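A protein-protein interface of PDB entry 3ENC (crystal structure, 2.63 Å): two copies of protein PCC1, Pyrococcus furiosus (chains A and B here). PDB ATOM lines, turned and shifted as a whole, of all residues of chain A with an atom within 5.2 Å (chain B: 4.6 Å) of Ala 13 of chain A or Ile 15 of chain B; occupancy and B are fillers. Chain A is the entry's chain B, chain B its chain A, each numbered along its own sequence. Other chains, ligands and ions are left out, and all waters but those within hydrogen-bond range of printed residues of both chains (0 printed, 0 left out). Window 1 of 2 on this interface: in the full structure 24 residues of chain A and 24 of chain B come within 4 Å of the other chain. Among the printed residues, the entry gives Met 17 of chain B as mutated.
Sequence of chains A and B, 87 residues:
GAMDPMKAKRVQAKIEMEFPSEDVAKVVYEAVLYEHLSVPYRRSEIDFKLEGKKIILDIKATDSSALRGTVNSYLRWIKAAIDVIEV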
ATOM      1  N   VAL A  11      25.043 -24.180   1.747  1.00  0.00           N
ATOM      2  CA  VAL A  11      26.083 -24.715   0.881  1.00  0.00           C
ATOM      3  C   VAL A  11      25.569 -25.786  -0.080  1.00  0.00           C
ATOM      4  O   VAL A  11      24.970 -26.775   0.332  1.00  0.00           O
ATOM      5  CB  VAL A  11      27.242 -25.269   1.705  1.00  0.00           C
ATOM      6  CG1 VAL A  11      27.802 -24.177   2.588  1.00  0.00           C
ATOM      7  CG2 VAL A  11      26.776 -26.444   2.540  1.00  0.00           C
ATOM      8  N   GLN A  12      25.827 -25.585  -1.368  1.00  0.00           N
ATOM      9  CA  GLN A  12      25.199 -26.384  -2.415  1.00  0.00           C
ATOM     10  C   GLN A  12      26.165 -26.850  -3.512  1.00  0.00           C
ATOM     11  O   GLN A  12      26.993 -26.076  -4.008  1.00  0.00           O
ATOM     12  CB  GLN A  12      24.032 -25.603  -3.032  1.00  0.00           C
ATOM     13  CG  GLN A  12      24.379 -24.190  -3.509  1.00  0.00           C
ATOM     14  CD  GLN A  12      24.476 -23.167  -2.375  1.00  0.00           C
ATOM     15  OE1 GLN A  12      24.188 -23.473  -1.217  1.00  0.00           O
ATOM     16  NE2 GLN A  12      24.876 -21.943  -2.713  1.00  0.00           N
ATOM     17  N   ALA A  13      26.043 -28.121  -3.888  1.00  0.00           N
ATOM     18  CA  ALA A  13      26.885 -28.712  -4.922  1.00  0.00           C
ATOM     19  C   ALA A  13      26.047 -29.458  -5.948  1.00  0.00           C
ATOM     20  O   ALA A  13      25.398 -30.442  -5.614  1.00  0.00           O
ATOM     21  CB  ALA A  13      27.898 -29.659  -4.298  1.00  0.00           C
ATOM     22  N   LYS A  14      26.067 -28.995  -7.195  1.00  0.00           N
ATOM     23  CA  LYS A  14      25.406 -29.708  -8.285  1.00  0.00           C
ATOM     24  C   LYS A  14      26.449 -30.530  -9.023  1.00  0.00           C
ATOM     25  O   LYS A  14      27.497 -30.016  -9.405  1.00  0.00           O
ATOM     26  CB  LYS A  14      24.713 -28.731  -9.247  1.00  0.00           C
ATOM     27  CG  LYS A  14      23.863 -29.378 -10.352  1.00  0.00           C
ATOM     28  CD  LYS A  14      22.960 -28.341 -11.044  1.00  0.00           C
ATOM     29  CE  LYS A  14      22.203 -28.927 -12.232  1.00  0.00           C
ATOM     30  NZ  LYS A  14      21.257 -27.932 -12.829  1.00  0.00           N
ATOM     31  N   ILE A  15      26.167 -31.811  -9.216  1.00  0.00           N
ATOM     32  CA  ILE A  15      27.113 -32.697  -9.878  1.00  0.00           C
ATOM     33  C   ILE A  15      26.500 -33.321 -11.121  1.00  0.00           C
ATOM     34  O   ILE A  15      25.295 -33.568 -11.155  1.00  0.00           O
ATOM     35  CB  ILE A  15      27.543 -33.832  -8.950  1.00  0.00           C
ATOM     36  CG1 ILE A  15      28.331 -33.284  -7.761  1.00  0.00           C
ATOM     37  CG2 ILE A  15      28.373 -34.839  -9.713  1.00  0.00           C
ATOM     38  CD1 ILE A  15      27.494 -32.562  -6.714  1.00  0.00           C
ATOM     39  N   LEU A  57      23.372 -35.164  -9.527  1.00  0.00           N
ATOM     40  CA  LEU A  57      23.207 -35.230  -8.080  1.00  0.00           C
ATOM     41  C   LEU A  57      23.182 -33.837  -7.455  1.00  0.00           C
ATOM     42  O   LEU A  57      24.224 -33.197  -7.298  1.00  0.00           O
ATOM     43  CB  LEU A  57      24.322 -36.059  -7.442  1.00  0.00           C
ATOM     44  CG  LEU A  57      24.333 -36.015  -5.908  1.00  0.00           C
ATOM     45  CD1 LEU A  57      22.939 -36.299  -5.366  1.00  0.00           C
ATOM     46  CD2 LEU A  57      25.352 -36.977  -5.300  1.00  0.00           C
ATOM     47  N   ASP A  58      21.982 -33.374  -7.112  1.00  0.00           N
ATOM     48  CA  ASP A  58      21.797 -32.092  -6.440  1.00  0.00           C
ATOM     49  C   ASP A  58      21.964 -32.300  -4.928  1.00  0.00           C
ATOM     50  O   ASP A  58      21.439 -33.269  -4.371  1.00  0.00           O
ATOM     51  CB  ASP A  58      20.409 -31.502  -6.759  1.00  0.00           C
ATOM     52  CG  ASP A  58      20.306 -30.935  -8.179  1.00  0.00           C
ATOM     53  OD1 ASP A  58      21.334 -30.476  -8.717  1.00  0.00           O
ATOM     54  OD2 ASP A  58      19.189 -30.932  -8.752  1.00  0.00           O
ATOM     55  N   ILE A  59      22.700 -31.401  -4.274  1.00  0.00           N
ATOM     56  CA  ILE A  59      22.994 -31.512  -2.847  1.00  0.00           C
ATOM     57  C   ILE A  59      22.879 -30.162  -2.164  1.00  0.00           C
ATOM     58  O   ILE A  59      23.655 -29.256  -2.458  1.00  0.00           O
ATOM     59  CB  ILE A  59      24.434 -32.007  -2.605  1.00  0.00           C
ATOM     60  CG1 ILE A  59      24.548 -33.516  -2.811  1.00  0.00           C
ATOM     61  CG2 ILE A  59      24.895 -31.644  -1.200  1.00  0.00           C
ATOM     62  CD1 ILE A  59      25.959 -33.959  -3.121  1.00  0.00           C
ATOM     63  N   LEU A  67      27.690 -30.606   3.592  1.00  0.00           N
ATOM     64  CA  LEU A  67      27.938 -30.785   2.174  1.00  0.00           C
ATOM     65  C   LEU A  67      28.987 -31.875   1.941  1.00  0.00           C
ATOM     66  O   LEU A  67      28.852 -32.684   1.031  1.00  0.00           O
ATOM     67  CB  LEU A  67      28.417 -29.465   1.567  1.00  0.00           C
ATOM     68  CG  LEU A  67      27.875 -29.102   0.187  1.00  0.00           C
ATOM     69  CD1 LEU A  67      28.576 -27.859  -0.342  1.00  0.00           C
ATOM     70  CD2 LEU A  67      28.012 -30.267  -0.774  1.00  0.00           C
ATOM     71  N   ALA B  13      31.961 -30.933 -10.948  1.00  0.00           N
ATOM     72  CA  ALA B  13      31.326 -30.529  -9.675  1.00  0.00           C
ATOM     73  C   ALA B  13      31.353 -29.011  -9.436  1.00  0.00           C
ATOM     74  O   ALA B  13      32.277 -28.327  -9.873  1.00  0.00           O
ATOM     75  CB  ALA B  13      31.975 -31.257  -8.495  1.00  0.00           C
ATOM     76  N   LYS B  14      30.352 -28.492  -8.727  1.00  0.00           N
ATOM     77  CA  LYS B  14      30.207 -27.050  -8.535  1.00  0.00           C
ATOM     78  C   LYS B  14      29.650 -26.766  -7.145  1.00  0.00           C
ATOM     79  O   LYS B  14      28.564 -27.229  -6.811  1.00  0.00           O
ATOM     80  CB  LYS B  14      29.269 -26.475  -9.607  1.00  0.00           C
ATOM     81  CG  LYS B  14      29.189 -24.940  -9.723  1.00  0.00           C
ATOM     82  CD  LYS B  14      28.422 -24.534 -11.000  1.00  0.00           C
ATOM     83  CE  LYS B  14      28.350 -23.023 -11.226  1.00  0.00           C
ATOM     84  NZ  LYS B  14      27.668 -22.686 -12.524  1.00  0.00           N
ATOM     85  N   ILE B  15      30.389 -26.010  -6.335  1.00  0.00           N
ATOM     86  CA  ILE B  15      29.903 -25.656  -5.010  1.00  0.00           C
ATOM     87  C   ILE B  15      29.846 -24.167  -4.764  1.00  0.00           C
ATOM     88  O   ILE B  15      30.791 -23.440  -5.069  1.00  0.00           O
ATOM     89  CB  ILE B  15      30.751 -26.263  -3.895  1.00  0.00           C
ATOM     90  CG1 ILE B  15      30.831 -27.779  -4.045  1.00  0.00           C
ATOM     91  CG2 ILE B  15      30.180 -25.856  -2.537  1.00  0.00           C
ATOM     92  CD1 ILE B  15      31.931 -28.223  -4.971  1.00  0.00           C
ATOM     93  N   GLU B  16      28.727 -23.726  -4.199  1.00  0.00           N
ATOM     94  CA  GLU B  16      28.563 -22.342  -3.791  1.00  0.00           C
ATOM     95  C   GLU B  16      28.384 -22.331  -2.289  1.00  0.00           C
ATOM     96  O   GLU B  16      27.823 -23.259  -1.729  1.00  0.00           O
ATOM     97  CB  GLU B  16      27.320 -21.741  -4.446  1.00  0.00           C
ATOM     98  CG  GLU B  16      27.243 -21.884  -5.965  1.00  0.00           C
ATOM     99  CD  GLU B  16      26.039 -21.150  -6.540  1.00  0.00           C
ATOM    100  OE1 GLU B  16      25.335 -20.463  -5.764  1.00  0.00           O
ATOM    101  OE2 GLU B  16      25.791 -21.254  -7.763  1.00  0.00           O
ATOM    102  N   MET B  17      28.840 -21.279  -1.629  1.00  0.00           N
ATOM    103  CA  MET B  17      28.650 -21.213  -0.193  1.00  0.00           C
ATOM    104  C   MET B  17      28.352 -19.835   0.325  1.00  0.00           C
ATOM    105  O   MET B  17      28.853 -18.835  -0.193  1.00  0.00           O
ATOM    106  CB  MET B  17      29.849 -21.766   0.538  1.00  0.00           C
ATOM    107  CG  MET B  17      30.082 -23.214   0.246  1.00  0.00           C
ATOM    108  SD  MET B  17      31.655 -23.608   1.215  1.00  0.00           S
ATOM    109  CE  MET B  17      31.108 -22.907   2.948  1.00  0.00           C
ATOM    110  N   ILE B  55      31.260 -18.210  -2.150  1.00  0.00           N
ATOM    111  CA  ILE B  55      32.519 -18.760  -2.602  1.00  0.00           C
ATOM    112  C   ILE B  55      32.185 -19.852  -3.598  1.00  0.00           C
ATOM    113  O   ILE B  55      31.444 -20.789  -3.282  1.00  0.00           O
ATOM    114  CB  ILE B  55      33.325 -19.345  -1.443  1.00  0.00           C
ATOM    115  CG1 ILE B  55      33.862 -18.240  -0.555  1.00  0.00           C
ATOM    116  CG2 ILE B  55      34.464 -20.129  -1.959  1.00  0.00           C
ATOM    117  CD1 ILE B  55      34.741 -18.765   0.540  1.00  0.00           C
ATOM    118  N   ILE B  56      32.723 -19.719  -4.806  1.00  0.00           N
ATOM    119  CA  ILE B  56      32.362 -20.601  -5.906  1.00  0.00           C
ATOM    120  C   ILE B  56      33.453 -21.587  -6.216  1.00  0.00           C
ATOM    121  O   ILE B  56      34.596 -21.212  -6.472  1.00  0.00           O
ATOM    122  CB  ILE B  56      32.129 -19.825  -7.197  1.00  0.00           C
ATOM    123  CG1 ILE B  56      31.320 -18.567  -6.912  1.00  0.00           C
ATOM    124  CG2 ILE B  56      31.471 -20.724  -8.241  1.00  0.00           C
ATOM    125  CD1 ILE B  56      30.146 -18.811  -6.003  1.00  0.00           C
ATOM    126  N   LEU B  57      33.080 -22.851  -6.236  1.00  0.00           N
ATOM    127  CA  LEU B  57      34.027 -23.897  -6.537  1.00  0.00           C
ATOM    128  C   LEU B  57      33.509 -24.756  -7.675  1.00  0.00           C
ATOM    129  O   LEU B  57      32.499 -25.437  -7.530  1.00  0.00           O
ATOM    130  CB  LEU B  57      34.257 -24.752  -5.299  1.00  0.00           C
ATOM    131  CG  LEU B  57      35.433 -25.706  -5.438  1.00  0.00           C
ATOM    132  CD1 LEU B  57      36.588 -24.975  -6.082  1.00  0.00           C
ATOM    133  CD2 LEU B  57      35.837 -26.279  -4.098  1.00  0.00           C
ATOM    134  N   ILE B  59      34.805 -27.815 -10.210  1.00  0.00           N
ATOM    135  CA  ILE B  59      35.886 -28.796 -10.343  1.00  0.00           C
ATOM    136  C   ILE B  59      35.681 -29.801 -11.499  1.00  0.00           C
ATOM    137  O   ILE B  59      34.627 -29.819 -12.134  1.00  0.00           O
ATOM    138  CB  ILE B  59      36.130 -29.545  -9.004  1.00  0.00           C
ATOM    139  CG1 ILE B  59      36.101 -28.582  -7.807  1.00  0.00           C
ATOM    140  CG2 ILE B  59      37.441 -30.295  -9.028  1.00  0.00           C
ATOM    141  CD1 ILE B  59      34.756 -28.502  -7.115  1.00  0.00           C
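Of the printed residues of chain B, Val 11 of chain A touches Glu 16 (3.5 Å) and Met 17 (3.4 Å). Of chain B, only Lys 14 (2.9 Å) and Ile 15 (3.5 Å) come within 4 Å of Ala 13 of chain A. Of the printed residues of chain A, Ala 13 of chain B touches Lys 14 (3.9 Å). Of the printed residues of chain A, Ile 15 of chain B touches Gln 12, Ala 13 and Leu 67. Of the printed residues of chain A, Met 17 of chain B touches Val 11 (3.4 Å).
Among the printed residues, pairs that only touch across the chains: Ala 13 of chain A with Lys 14 of chain B (2.9 Å), Gln 12 of chain A with Ile 15 of chain B (3.1 Å), Leu 67 of chain A with Ile 15 of chain B (3.4 Å), Val 11 of chain A with Met 17 of chain B (3.4 Å), Val 11 of chain A with Glu 16 of chain B (3.5 Å), Ala 13 of chain A with Ile 15 of chain B (3.5 Å) and Lys 14 of chain A with Ala 13 of chain B (3.9 Å).
Of the 9 printed residues of chain A, 5 touch a printed residue of chain B. Of the 9 printed residues of chain B, 5 touch a printed residue of chain A. Hydrophobic or aromatic side chains of chain B that line the printed part of chain A: Ile 15 and Met 17.
Ala 13 of chain A touches Lys 14 of chain B, and with the chains exchanged Lys 14 of chain A touches Ala 13 of chain B. Ala 13 of chain A touches Ile 15 of chain B, but with the chains exchanged Ile 15 of chain A does not touch Ala 13 of chain B (4.2 Å). Lys 14 of chain B touches its own counterpart, Lys 14 of chain A.
The backbone carbonyl oxygen (O) of Ala 13 of chain B sits at hydrogen-bond distance from the backbone NH (N) of Ile 59 of chain B (2.6 Å). The backbone carbonyl oxygen (O) of Leu 57 of chain B is in hydrogen-bond range of the backbone NH (N) of Ile 15 of chain B (2.5 Å). O of Ile 55 of chain B lies within hydrogen-bond range of N of Met 17 of chain B, at 3.1 Å. N of Ala 13 of chain A is in hydrogen-bond range of O of Ile 59 of chain A.
The backbone carbonyl oxygen (O) of Lys 14 of chain B lies within hydrogen-bond range of the backbone NH (N) of Lys 14 of chain A (3.1 Å). The backbone carbonyl oxygen (O) of Gln 12 of chain A is in hydrogen-bond range of the backbone NH (N) of Glu 16 of chain B (2.9 Å). The backbone carbonyl oxygen of Lys 14 of chain B sits close to the backbone carbonyl oxygen of Gln 12 of chain A.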
